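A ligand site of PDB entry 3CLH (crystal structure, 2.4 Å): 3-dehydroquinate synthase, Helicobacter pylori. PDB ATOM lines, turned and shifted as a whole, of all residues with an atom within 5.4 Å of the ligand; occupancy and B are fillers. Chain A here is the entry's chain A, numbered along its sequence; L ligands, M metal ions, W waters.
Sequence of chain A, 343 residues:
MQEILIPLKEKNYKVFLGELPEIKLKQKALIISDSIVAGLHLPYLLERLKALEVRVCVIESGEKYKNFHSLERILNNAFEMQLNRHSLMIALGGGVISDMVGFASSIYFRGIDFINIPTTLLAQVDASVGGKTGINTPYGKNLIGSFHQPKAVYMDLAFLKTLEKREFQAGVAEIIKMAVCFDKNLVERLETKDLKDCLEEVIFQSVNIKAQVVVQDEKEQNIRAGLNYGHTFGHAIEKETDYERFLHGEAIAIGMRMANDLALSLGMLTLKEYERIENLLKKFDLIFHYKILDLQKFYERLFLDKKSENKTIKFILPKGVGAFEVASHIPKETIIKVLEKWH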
ATOM      1  N   ASP A  34      25.393  12.663  15.008  1.00  0.00           N
ATOM      2  CA  ASP A  34      25.567  12.573  16.456  1.00  0.00           C
ATOM      3  C   ASP A  34      24.540  11.633  17.101  1.00  0.00           C
ATOM      4  O   ASP A  34      23.589  11.211  16.441  1.00  0.00           O
ATOM      5  CB  ASP A  34      25.564  13.961  17.120  1.00  0.00           C
ATOM      6  CG  ASP A  34      24.246  14.693  16.956  1.00  0.00           C
ATOM      7  OD1 ASP A  34      23.227  14.254  17.531  1.00  0.00           O
ATOM      8  OD2 ASP A  34      24.237  15.746  16.272  1.00  0.00           O
ATOM      9  N   ILE A  36      22.096  11.976  19.236  1.00  0.00           N
ATOM     10  CA  ILE A  36      20.702  12.415  19.304  1.00  0.00           C
ATOM     11  C   ILE A  36      20.033  12.420  17.924  1.00  0.00           C
ATOM     12  O   ILE A  36      18.902  11.953  17.776  1.00  0.00           O
ATOM     13  CB  ILE A  36      20.559  13.803  20.004  1.00  0.00           C
ATOM     14  CG1 ILE A  36      21.187  13.770  21.396  1.00  0.00           C
ATOM     15  CG2 ILE A  36      19.085  14.223  20.099  1.00  0.00           C
ATOM     16  CD1 ILE A  36      21.240  15.106  22.128  1.00  0.00           C
ATOM     17  N   VAL A  37      20.736  12.943  16.915  1.00  0.00           N
ATOM     18  CA  VAL A  37      20.214  13.030  15.554  1.00  0.00           C
ATOM     19  C   VAL A  37      20.051  11.648  14.902  1.00  0.00           C
ATOM     20  O   VAL A  37      19.090  11.416  14.162  1.00  0.00           O
ATOM     21  CB  VAL A  37      21.100  13.948  14.655  1.00  0.00           C
ATOM     22  CG1 VAL A  37      20.613  13.956  13.207  1.00  0.00           C
ATOM     23  CG2 VAL A  37      21.107  15.369  15.192  1.00  0.00           C
ATOM     24  N   LEU A  40      16.782   9.972  15.622  1.00  0.00           N
ATOM     25  CA  LEU A  40      15.627  10.802  15.272  1.00  0.00           C
ATOM     26  C   LEU A  40      15.468  11.034  13.772  1.00  0.00           C
ATOM     27  O   LEU A  40      14.351  10.956  13.244  1.00  0.00           O
ATOM     28  CB  LEU A  40      15.686  12.155  16.005  1.00  0.00           C
ATOM     29  CG  LEU A  40      15.438  12.218  17.517  1.00  0.00           C
ATOM     30  CD1 LEU A  40      15.876  13.559  18.077  1.00  0.00           C
ATOM     31  CD2 LEU A  40      13.970  11.947  17.853  1.00  0.00           C
ATOM     32  N   HIS A  41      16.576  11.291  13.085  1.00  0.00           N
ATOM     33  CA  HIS A  41      16.529  11.727  11.687  1.00  0.00           C
ATOM     34  C   HIS A  41      17.408  10.935  10.716  1.00  0.00           C
ATOM     35  O   HIS A  41      17.466  11.254   9.520  1.00  0.00           O
ATOM     36  CB  HIS A  41      16.856  13.223  11.584  1.00  0.00           C
ATOM     37  CG  HIS A  41      15.927  14.101  12.374  1.00  0.00           C
ATOM     38  ND1 HIS A  41      14.586  14.218  12.069  1.00  0.00           N
ATOM     39  CD2 HIS A  41      16.144  14.895  13.446  1.00  0.00           C
ATOM     40  CE1 HIS A  41      14.022  15.060  12.923  1.00  0.00           C
ATOM     41  NE2 HIS A  41      14.949  15.482  13.762  1.00  0.00           N
ATOM     42  N   SER A  61      27.050  13.437  21.111  1.00  0.00           N
ATOM     43  CA  SER A  61      26.492  14.792  21.063  1.00  0.00           C
ATOM     44  C   SER A  61      27.158  15.734  22.062  1.00  0.00           C
ATOM     45  O   SER A  61      27.382  15.369  23.214  1.00  0.00           O
ATOM     46  CB  SER A  61      24.976  14.740  21.312  1.00  0.00           C
ATOM     47  OG  SER A  61      24.438  16.048  21.410  1.00  0.00           O
ATOM     48  N   GLY A  62      27.463  16.946  21.595  1.00  0.00           N
ATOM     49  CA  GLY A  62      28.060  17.969  22.444  1.00  0.00           C
ATOM     50  C   GLY A  62      29.148  18.795  21.792  1.00  0.00           C
ATOM     51  O   GLY A  62      29.744  18.380  20.785  1.00  0.00           O
ATOM     52  N   GLU A  63      29.410  19.965  22.361  1.00  0.00           N
ATOM     53  CA  GLU A  63      30.455  20.876  21.889  1.00  0.00           C
ATOM     54  C   GLU A  63      31.845  20.353  22.282  1.00  0.00           C
ATOM     55  O   GLU A  63      32.823  20.589  21.577  1.00  0.00           O
ATOM     56  CB  GLU A  63      30.230  22.286  22.455  1.00  0.00           C
ATOM     57  CG  GLU A  63      31.276  23.342  22.075  1.00  0.00           C
ATOM     58  CD  GLU A  63      31.236  23.723  20.594  1.00  0.00           C
ATOM     59  OE1 GLU A  63      30.133  23.786  20.014  1.00  0.00           O
ATOM     60  OE2 GLU A  63      32.319  23.972  20.027  1.00  0.00           O
ATOM     61  N   LYS A  66      33.895  18.266  19.756  1.00  0.00           N
ATOM     62  CA  LYS A  66      34.415  18.937  18.563  1.00  0.00           C
ATOM     63  C   LYS A  66      35.934  19.099  18.701  1.00  0.00           C
ATOM     64  O   LYS A  66      36.436  20.198  18.967  1.00  0.00           O
ATOM     65  CB  LYS A  66      33.732  20.296  18.361  1.00  0.00           C
ATOM     66  CG  LYS A  66      33.910  20.894  16.978  1.00  0.00           C
ATOM     67  CD  LYS A  66      33.236  22.256  16.884  1.00  0.00           C
ATOM     68  CE  LYS A  66      33.510  22.900  15.537  1.00  0.00           C
ATOM     69  NZ  LYS A  66      32.825  24.219  15.405  1.00  0.00           N
ATOM     70  N   GLY A  93      23.625  16.706  10.963  1.00  0.00           N
ATOM     71  CA  GLY A  93      23.621  17.245  12.321  1.00  0.00           C
ATOM     72  C   GLY A  93      23.719  18.755  12.358  1.00  0.00           C
ATOM     73  O   GLY A  93      23.449  19.426  11.358  1.00  0.00           O
ATOM     74  N   GLY A  94      24.101  19.294  13.514  1.00  0.00           N
ATOM     75  CA  GLY A  94      24.234  20.738  13.695  1.00  0.00           C
ATOM     76  C   GLY A  94      25.519  21.309  13.130  1.00  0.00           C
ATOM     77  O   GLY A  94      26.132  20.725  12.232  1.00  0.00           O
ATOM     78  N   GLY A  95      25.926  22.452  13.667  1.00  0.00           N
ATOM     79  CA  GLY A  95      27.144  23.139  13.227  1.00  0.00           C
ATOM     80  C   GLY A  95      28.418  22.430  13.650  1.00  0.00           C
ATOM     81  O   GLY A  95      29.453  22.584  13.001  1.00  0.00           O
ATOM     82  N   VAL A  96      28.341  21.661  14.737  1.00  0.00           N
ATOM     83  CA  VAL A  96      29.476  20.894  15.240  1.00  0.00           C
ATOM     84  C   VAL A  96      29.833  19.749  14.283  1.00  0.00           C
ATOM     85  O   VAL A  96      31.018  19.521  14.001  1.00  0.00           O
ATOM     86  CB  VAL A  96      29.202  20.358  16.675  1.00  0.00           C
ATOM     87  CG1 VAL A  96      30.277  19.374  17.124  1.00  0.00           C
ATOM     88  CG2 VAL A  96      29.089  21.512  17.667  1.00  0.00           C
ATOM     89  N   ILE A  97      28.822  19.050  13.792  1.00  0.00           N
ATOM     90  CA  ILE A  97      29.003  17.933  12.864  1.00  0.00           C
ATOM     91  C   ILE A  97      29.513  18.417  11.504  1.00  0.00           C
ATOM     92  O   ILE A  97      30.492  17.887  10.978  1.00  0.00           O
ATOM     93  CB  ILE A  97      27.688  17.099  12.695  1.00  0.00           C
ATOM     94  CG1 ILE A  97      27.140  16.637  14.055  1.00  0.00           C
ATOM     95  CG2 ILE A  97      27.904  15.913  11.740  1.00  0.00           C
ATOM     96  CD1 ILE A  97      28.073  15.756  14.881  1.00  0.00           C
ATOM     97  N   ASP A  99      31.109  21.135  10.625  1.00  0.00           N
ATOM     98  CA  ASP A  99      32.477  21.652  10.698  1.00  0.00           C
ATOM     99  C   ASP A  99      33.515  20.540  10.779  1.00  0.00           C
ATOM    100  O   ASP A  99      34.607  20.653  10.219  1.00  0.00           O
ATOM    101  CB  ASP A  99      32.639  22.606  11.895  1.00  0.00           C
ATOM    102  CG  ASP A  99      32.010  23.969  11.651  1.00  0.00           C
ATOM    103  OD1 ASP A  99      31.167  24.098  10.740  1.00  0.00           O
ATOM    104  OD2 ASP A  99      32.359  24.919  12.387  1.00  0.00           O
ATOM    105  N   THR A 119      20.580  20.139  10.600  1.00  0.00           N
ATOM    106  CA  THR A 119      19.366  19.798  11.348  1.00  0.00           C
ATOM    107  C   THR A 119      18.941  20.908  12.307  1.00  0.00           C
ATOM    108  O   THR A 119      17.741  21.060  12.592  1.00  0.00           O
ATOM    109  CB  THR A 119      19.518  18.473  12.126  1.00  0.00           C
ATOM    110  OG1 THR A 119      20.618  18.570  13.043  1.00  0.00           O
ATOM    111  CG2 THR A 119      19.741  17.297  11.180  1.00  0.00           C
ATOM    112  N   THR A 120      19.911  21.674  12.810  1.00  0.00           N
ATOM    113  CA  THR A 120      19.625  22.812  13.678  1.00  0.00           C
ATOM    114  C   THR A 120      19.320  24.071  12.855  1.00  0.00           C
ATOM    115  O   THR A 120      19.747  24.178  11.710  1.00  0.00           O
ATOM    116  CB  THR A 120      20.798  23.120  14.646  1.00  0.00           C
ATOM    117  OG1 THR A 120      22.010  23.280  13.905  1.00  0.00           O
ATOM    118  CG2 THR A 120      20.977  22.004  15.661  1.00  0.00           C
ATOM    119  N   LEU A 122      20.420  27.057  13.575  1.00  0.00           N
ATOM    120  CA  LEU A 122      21.695  27.782  13.509  1.00  0.00           C
ATOM    121  C   LEU A 122      22.539  27.330  12.318  1.00  0.00           C
ATOM    122  O   LEU A 122      23.106  28.163  11.612  1.00  0.00           O
ATOM    123  CB  LEU A 122      22.469  27.592  14.829  1.00  0.00           C
ATOM    124  CG  LEU A 122      23.879  28.157  15.075  1.00  0.00           C
ATOM    125  CD1 LEU A 122      24.968  27.266  14.474  1.00  0.00           C
ATOM    126  CD2 LEU A 122      24.039  29.605  14.615  1.00  0.00           C
ATOM    127  N   ALA A 123      22.603  26.013  12.094  1.00  0.00           N
ATOM    128  CA  ALA A 123      23.391  25.447  10.999  1.00  0.00           C
ATOM    129  C   ALA A 123      22.758  25.687   9.633  1.00  0.00           C
ATOM    130  O   ALA A 123      23.460  25.729   8.621  1.00  0.00           O
ATOM    131  CB  ALA A 123      23.642  23.966  11.233  1.00  0.00           C
ATOM    132  N   ASP A 126      23.587  29.734   9.088  1.00  0.00           N
ATOM    133  CA  ASP A 126      24.933  30.259   9.294  1.00  0.00           C
ATOM    134  C   ASP A 126      26.058  29.278   8.922  1.00  0.00           C
ATOM    135  O   ASP A 126      26.968  29.633   8.176  1.00  0.00           O
ATOM    136  CB  ASP A 126      25.107  30.744  10.745  1.00  0.00           C
ATOM    137  CG  ASP A 126      26.289  31.690  10.913  1.00  0.00           C
ATOM    138  OD1 ASP A 126      26.764  32.264   9.907  1.00  0.00           O
ATOM    139  OD2 ASP A 126      26.736  31.876  12.061  1.00  0.00           O
ATOM    140  N   ALA A 127      25.977  28.051   9.442  1.00  0.00           N
ATOM    141  CA  ALA A 127      27.051  27.062   9.277  1.00  0.00           C
ATOM    142  C   ALA A 127      27.091  26.397   7.898  1.00  0.00           C
ATOM    143  O   ALA A 127      28.153  25.953   7.451  1.00  0.00           O
ATOM    144  CB  ALA A 127      26.984  26.007  10.378  1.00  0.00           C
ATOM    145  N   SER A 128      25.940  26.328   7.231  1.00  0.00           N
ATOM    146  CA  SER A 128      25.814  25.671   5.931  1.00  0.00           C
ATOM    147  C   SER A 128      26.549  26.425   4.816  1.00  0.00           C
ATOM    148  O   SER A 128      27.395  25.845   4.130  1.00  0.00           O
ATOM    149  CB  SER A 128      24.340  25.496   5.554  1.00  0.00           C
ATOM    150  OG  SER A 128      23.648  26.733   5.614  1.00  0.00           O
ATOM    151  N   LYS A 132      33.480  27.589   5.847  1.00  0.00           N
ATOM    152  CA  LYS A 132      34.287  27.535   7.061  1.00  0.00           C
ATOM    153  C   LYS A 132      34.098  26.222   7.821  1.00  0.00           C
ATOM    154  O   LYS A 132      32.979  25.902   8.248  1.00  0.00           O
ATOM    155  CB  LYS A 132      33.986  28.727   7.972  1.00  0.00           C
ATOM    156  CG  LYS A 132      34.509  30.057   7.470  1.00  0.00           C
ATOM    157  CD  LYS A 132      34.220  31.171   8.474  1.00  0.00           C
ATOM    158  CE  LYS A 132      34.806  32.497   8.015  1.00  0.00           C
ATOM    159  NZ  LYS A 132      34.522  33.592   8.978  1.00  0.00           N
ATOM    160  N   THR A 133      35.180  25.477   7.960  1.00  0.00           N
ATOM    161  CA  THR A 133      35.176  24.201   8.682  1.00  0.00           C
ATOM    162  C   THR A 133      36.279  24.195   9.736  1.00  0.00           C
ATOM    163  O   THR A 133      37.190  25.027   9.689  1.00  0.00           O
ATOM    164  CB  THR A 133      35.377  22.997   7.724  1.00  0.00           C
ATOM    165  OG1 THR A 133      36.660  23.084   7.088  1.00  0.00           O
ATOM    166  CG2 THR A 133      34.288  22.973   6.647  1.00  0.00           C
ATOM    167  N   ASN A 136      37.953  22.268  17.564  1.00  0.00           N
ATOM    168  CA  ASN A 136      38.474  23.007  18.705  1.00  0.00           C
ATOM    169  C   ASN A 136      39.777  22.418  19.255  1.00  0.00           C
ATOM    170  O   ASN A 136      39.971  21.199  19.230  1.00  0.00           O
ATOM    171  CB  ASN A 136      37.427  23.090  19.831  1.00  0.00           C
ATOM    172  CG  ASN A 136      36.141  23.779  19.390  1.00  0.00           C
ATOM    173  OD1 ASN A 136      36.103  24.462  18.362  1.00  0.00           O
ATOM    174  ND2 ASN A 136      35.084  23.597  20.169  1.00  0.00           N
ATOM    175  N   ASN A 142      37.830  26.751  16.980  1.00  0.00           N
ATOM    176  CA  ASN A 142      37.904  26.976  15.528  1.00  0.00           C
ATOM    177  C   ASN A 142      39.221  27.587  15.037  1.00  0.00           C
ATOM    178  O   ASN A 142      39.224  28.452  14.149  1.00  0.00           O
ATOM    179  CB  ASN A 142      36.700  27.797  15.035  1.00  0.00           C
ATOM    180  CG  ASN A 142      35.372  27.126  15.333  1.00  0.00           C
ATOM    181  OD1 ASN A 142      35.186  25.932  15.091  1.00  0.00           O
ATOM    182  ND2 ASN A 142      34.421  27.901  15.856  1.00  0.00           N
ATOM    183  N   PHE A 159      13.463  18.588  10.191  1.00  0.00           N
ATOM    184  CA  PHE A 159      14.459  18.327  11.232  1.00  0.00           C
ATOM    185  C   PHE A 159      14.363  19.340  12.383  1.00  0.00           C
ATOM    186  O   PHE A 159      14.785  19.038  13.506  1.00  0.00           O
ATOM    187  CB  PHE A 159      15.882  18.347  10.648  1.00  0.00           C
ATOM    188  CG  PHE A 159      16.091  17.393   9.506  1.00  0.00           C
ATOM    189  CD1 PHE A 159      15.704  16.059   9.605  1.00  0.00           C
ATOM    190  CD2 PHE A 159      16.705  17.824   8.335  1.00  0.00           C
ATOM    191  CE1 PHE A 159      15.911  15.169   8.555  1.00  0.00           C
ATOM    192  CE2 PHE A 159      16.914  16.940   7.276  1.00  0.00           C
ATOM    193  CZ  PHE A 159      16.523  15.613   7.381  1.00  0.00           C
ATOM    194  N   LEU A 160      13.808  20.506  12.091  1.00  0.00           N
ATOM    195  CA  LEU A 160      13.715  21.609  13.056  1.00  0.00           C
ATOM    196  C   LEU A 160      12.639  21.401  14.123  1.00  0.00           C
ATOM    197  O   LEU A 160      12.664  22.038  15.175  1.00  0.00           O
ATOM    198  CB  LEU A 160      13.478  22.941  12.340  1.00  0.00           C
ATOM    199  CG  LEU A 160      14.428  23.386  11.218  1.00  0.00           C
ATOM    200  CD1 LEU A 160      13.864  24.603  10.501  1.00  0.00           C
ATOM    201  CD2 LEU A 160      15.823  23.686  11.752  1.00  0.00           C
ATOM    202  N   THR A 162      11.978  18.733  15.965  1.00  0.00           N
ATOM    203  CA  THR A 162      12.427  17.960  17.122  1.00  0.00           C
ATOM    204  C   THR A 162      13.340  18.752  18.067  1.00  0.00           C
ATOM    205  O   THR A 162      13.656  18.295  19.167  1.00  0.00           O
ATOM    206  CB  THR A 162      13.141  16.665  16.693  1.00  0.00           C
ATOM    207  OG1 THR A 162      14.181  16.981  15.762  1.00  0.00           O
ATOM    208  CG2 THR A 162      12.169  15.681  16.052  1.00  0.00           C
ATOM    209  N   LEU A 163      13.754  19.937  17.616  1.00  0.00           N
ATOM    210  CA  LEU A 163      14.630  20.815  18.406  1.00  0.00           C
ATOM    211  C   LEU A 163      13.940  21.350  19.656  1.00  0.00           C
ATOM    212  O   LEU A 163      12.725  21.574  19.660  1.00  0.00           O
ATOM    213  CB  LEU A 163      15.133  21.977  17.545  1.00  0.00           C
ATOM    214  CG  LEU A 163      16.200  21.713  16.494  1.00  0.00           C
ATOM    215  CD1 LEU A 163      16.309  22.894  15.539  1.00  0.00           C
ATOM    216  CD2 LEU A 163      17.556  21.423  17.126  1.00  0.00           C
ATOM    217  N   GLU A 164      14.734  21.561  20.708  1.00  0.00           N
ATOM    218  CA  GLU A 164      14.245  22.176  21.943  1.00  0.00           C
ATOM    219  C   GLU A 164      13.985  23.660  21.736  1.00  0.00           C
ATOM    220  O   GLU A 164      14.523  24.272  20.808  1.00  0.00           O
ATOM    221  CB  GLU A 164      15.263  21.969  23.083  1.00  0.00           C
ATOM    222  CG  GLU A 164      15.520  20.503  23.459  1.00  0.00           C
ATOM    223  CD  GLU A 164      14.380  19.872  24.264  1.00  0.00           C
ATOM    224  OE1 GLU A 164      13.605  20.618  24.900  1.00  0.00           O
ATOM    225  OE2 GLU A 164      14.281  18.629  24.264  1.00  0.00           O
ATOM    226  N   GLU A 167      17.224  25.827  22.047  1.00  0.00           N
ATOM    227  CA  GLU A 167      18.112  25.673  20.897  1.00  0.00           C
ATOM    228  C   GLU A 167      17.565  26.354  19.641  1.00  0.00           C
ATOM    229  O   GLU A 167      18.340  26.814  18.797  1.00  0.00           O
ATOM    230  CB  GLU A 167      18.357  24.184  20.606  1.00  0.00           C
ATOM    231  CG  GLU A 167      19.305  23.489  21.586  1.00  0.00           C
ATOM    232  CD  GLU A 167      20.771  23.884  21.402  1.00  0.00           C
ATOM    233  OE1 GLU A 167      21.153  24.291  20.275  1.00  0.00           O
ATOM    234  OE2 GLU A 167      21.539  23.764  22.377  1.00  0.00           O
HETATM  235  P1  LIG L   1      25.300  21.768  18.010  1.00  0.00           P
HETATM  236  O1  LIG L   1      25.809  21.305  16.695  1.00  0.00           O
HETATM  237  O2  LIG L   1      26.093  21.200  19.115  1.00  0.00           O
HETATM  238  O3  LIG L   1      23.744  21.381  18.164  1.00  0.00           O
HETATM  239  C1  LIG L   1      23.062  21.627  19.374  1.00  0.00           C
HETATM  240  C2  LIG L   1      22.560  20.331  20.022  1.00  0.00           C
HETATM  241  O4  LIG L   1      21.266  20.013  19.523  1.00  0.00           O
HETATM  242  C3  LIG L   1      23.466  19.135  19.760  1.00  0.00           C
HETATM  243  O5  LIG L   1      23.963  18.652  20.990  1.00  0.00           O
HETATM  244  C4  LIG L   1      22.597  18.105  19.068  1.00  0.00           C
HETATM  245  O6  LIG L   1      22.681  16.837  19.676  1.00  0.00           O
HETATM  246  C5  LIG L   1      21.179  18.640  19.172  1.00  0.00           C
HETATM  247  N1  LIG L   1      20.449  18.496  17.896  1.00  0.00           N
HETATM  248  C6  LIG L   1      20.934  18.728  16.639  1.00  0.00           C
HETATM  249  N2  LIG L   1      19.950  18.483  15.744  1.00  0.00           N
HETATM  250  C7  LIG L   1      18.839  18.097  16.403  1.00  0.00           C
HETATM  251  C8  LIG L   1      17.566  17.735  15.975  1.00  0.00           C
HETATM  252  N3  LIG L   1      17.208  17.942  14.717  1.00  0.00           N
HETATM  253  N4  LIG L   1      16.609  17.371  16.915  1.00  0.00           N
HETATM  254  C9  LIG L   1      16.918  17.379  18.265  1.00  0.00           C
HETATM  255  N5  LIG L   1      18.184  17.751  18.675  1.00  0.00           N
HETATM  256  C10 LIG L   1      19.134  18.098  17.771  1.00  0.00           C
HETATM  257  O7  LIG L   1      25.311  23.375  18.078  1.00  0.00           O
HETATM  258  P2  LIG L   1      24.919  24.304  16.821  1.00  0.00           P
HETATM  259  O8  LIG L   1      24.159  23.507  15.838  1.00  0.00           O
HETATM  260  O9  LIG L   1      24.335  25.559  17.349  1.00  0.00           O
HETATM  261  O10 LIG L   1      26.371  24.641  16.175  1.00  0.00           O
HETATM  262  C11 LIG L   1      27.308  25.437  16.865  1.00  0.00           C
HETATM  263  C12 LIG L   1      28.717  25.152  16.355  1.00  0.00           C
HETATM  264  O11 LIG L   1      28.789  25.394  14.968  1.00  0.00           O
HETATM  265  C13 LIG L   1      29.736  26.051  17.049  1.00  0.00           C
HETATM  266  O12 LIG L   1      30.656  25.268  17.772  1.00  0.00           O
HETATM  267  C14 LIG L   1      30.423  26.825  15.932  1.00  0.00           C
HETATM  268  O13 LIG L   1      31.828  26.700  16.004  1.00  0.00           O
HETATM  269  C15 LIG L   1      29.901  26.207  14.631  1.00  0.00           C
HETATM  270  N6  LIG L   1      29.520  27.261  13.659  1.00  0.00           N
HETATM  271  C16 LIG L   1      30.244  27.395  12.504  1.00  0.00           C
HETATM  272  C17 LIG L   1      29.906  28.367  11.561  1.00  0.00           C
HETATM  273  C18 LIG L   1      30.538  28.344  10.203  1.00  0.00           C
HETATM  274  O14 LIG L   1      30.508  27.148   9.459  1.00  0.00           O
HETATM  275  N7  LIG L   1      31.104  29.453   9.734  1.00  0.00           N
HETATM  276  C19 LIG L   1      28.821  29.206  11.809  1.00  0.00           C
HETATM  277  C20 LIG L   1      28.082  29.065  12.982  1.00  0.00           C
HETATM  278  C21 LIG L   1      28.442  28.079  13.903  1.00  0.00           C
HETATM  279 ZN    ZN M   1      29.510  29.814  16.799  1.00  0.00          ZN
HETATM  280  O   HOH W   1      24.927  20.088  23.242  1.00  0.00           O
HETATM  281  O   HOH W   2      24.283  17.025  23.987  1.00  0.00           O
HETATM  282  O   HOH W   3      24.197  25.115  20.040  1.00  0.00           O
HETATM  283  O   HOH W   4      30.766  28.835   6.978  1.00  0.00           O
HETATM  284  O   HOH W   5      21.659  24.855  17.517  1.00  0.00           O
HETATM  285  O   HOH W   6      33.097  26.442  18.413  1.00  0.00           O
HETATM  286  O   HOH W   7      25.215  18.332  16.380  1.00  0.00           O
HETATM  287  O   HOH W   8      29.840  23.997   8.344  1.00  0.00           O
HETATM  288  O   HOH W   9      32.756  29.381  13.465  1.00  0.00           O
HETATM  289  O   HOH W  10      18.685  18.005  21.502  1.00  0.00           O
HETATM  290  O   HOH W  11      27.527  28.871  17.097  1.00  0.00           O
HETATM  291  O   HOH W  12      25.324  27.425  19.085  1.00  0.00           O
HETATM  292  O   HOH W  13      27.297  18.735  19.084  1.00  0.00           O
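Water W3 bridges an oxygen (O9) of the ligand and the side-chain carboxylate of Glu 167. Water W6 lies within hydrogen-bond range of O13 of the ligand (2.7 Å), OE2 of Glu 63 (3.1 Å) and ND2 of Asn 142 (3.2 Å). Water W13 bridges an oxygen (O2) of the ligand (2.7 Å) and the backbone carbonyl oxygen (O) of Gly 62 (3.0 Å). Water W5 lies within hydrogen-bond range of an oxygen (O9) of the ligand (2.8 Å) and the side-chain carboxylate (OE1) of Glu 167 (2.9 Å). Water W7 lies within hydrogen-bond range of OD2 of Asp 34 (2.8 Å), O1 of the ligand (3.0 Å) and N of Gly 94 (3.2 Å). Water W2 bridges OG of Ser 61 (2.8 Å) and O5 of the ligand (3.4 Å).
The side-chain carboxylate of Asp 34 is in hydrogen-bond range of the backbone NH of Val 37 (2.9 Å). The backbone NH (N) of Ile 36 is in hydrogen-bond range of the side-chain carboxylate (OD1) of Asp 34. OD1 of Asn 142 is in hydrogen-bond range of NZ of Lys 66 (2.9 Å). The side-chain hydroxyl (OG1) of Thr 120 lies close to the backbone NH (N) of Ala 123 (3.3 Å). O of Lys 66 sits at hydrogen-bond distance from N of Asn 136. OD2 of Asp 99 lies within salt-bridge range of NZ of Lys 66 (3.1 Å). The side-chain amide oxygen of Asn 136 lies within hydrogen-bond range of the backbone NH of Asn 142, at 3.2 Å. NE2 of His 41 is in hydrogen-bond range of OG1 of Thr 162, at 2.6 Å.
The side-chain carboxylate (OD1) of Asp 99 lies close to an oxygen (O14) of the ligand. O14 of the ligand sits close to O of Ala 127. An oxygen (O14) of the ligand lies close to the backbone carbonyl oxygen of Lys 132, 3.0 Å away. Residues that only touch the ligand: Asp 126, Ile 36, Val 37, Glu 167, Leu 122, Gly 94, Leu 163, Gly 62 and Leu 40. Within 4 Å of the ligand: Asp 34, Ile 36, Val 37, Leu 40, His 41, Ser 61, Gly 62, Glu 63, Lys 66, Gly 94, Gly 95, Val 96, Asp 99, Thr 119, Thr 120, Leu 122, Asp 126, Ala 127, Lys 132, Asn 142, Phe 159, Thr 162, Leu 163 and Glu 167. The nearest printed residue that does not touch the ligand is Ala 123 (4.7 Å).
OE1 of Glu 63 is in hydrogen-bond range of O12 of the ligand (2.7 Å). O of Phe 159 is in hydrogen-bond range of N3 of the ligand, at 2.9 Å. The side-chain amino group (NZ) of Lys 66 sits at hydrogen-bond distance from an oxygen (O13) of the ligand. OG1 of Thr 162 lies within hydrogen-bond range of N4 of the ligand (2.7 Å). NE2 of His 41 lies close to N3 of the ligand (3.5 Å). The side-chain amide nitrogen (ND2) of Asn 142 is in hydrogen-bond range of an oxygen (O13) of the ligand (2.9 Å). A nitrogen (N2) of the ligand sits at hydrogen-bond distance from the side-chain hydroxyl of Thr 119 (2.8 Å). The side-chain hydroxyl of Ser 61 sits at hydrogen-bond distance from an oxygen (O6) of the ligand, at 2.6 Å. An oxygen (O6) of the ligand lies within hydrogen-bond range of the side-chain carboxylate of Asp 34. The side-chain hydroxyl of Thr 120 is in hydrogen-bond range of an oxygen (O8) of the ligand (2.9 Å). N of Gly 95 lies within hydrogen-bond range of O8 of the ligand. N of Val 96 lies within hydrogen-bond range of O1 of the ligand, 3.2 Å away.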
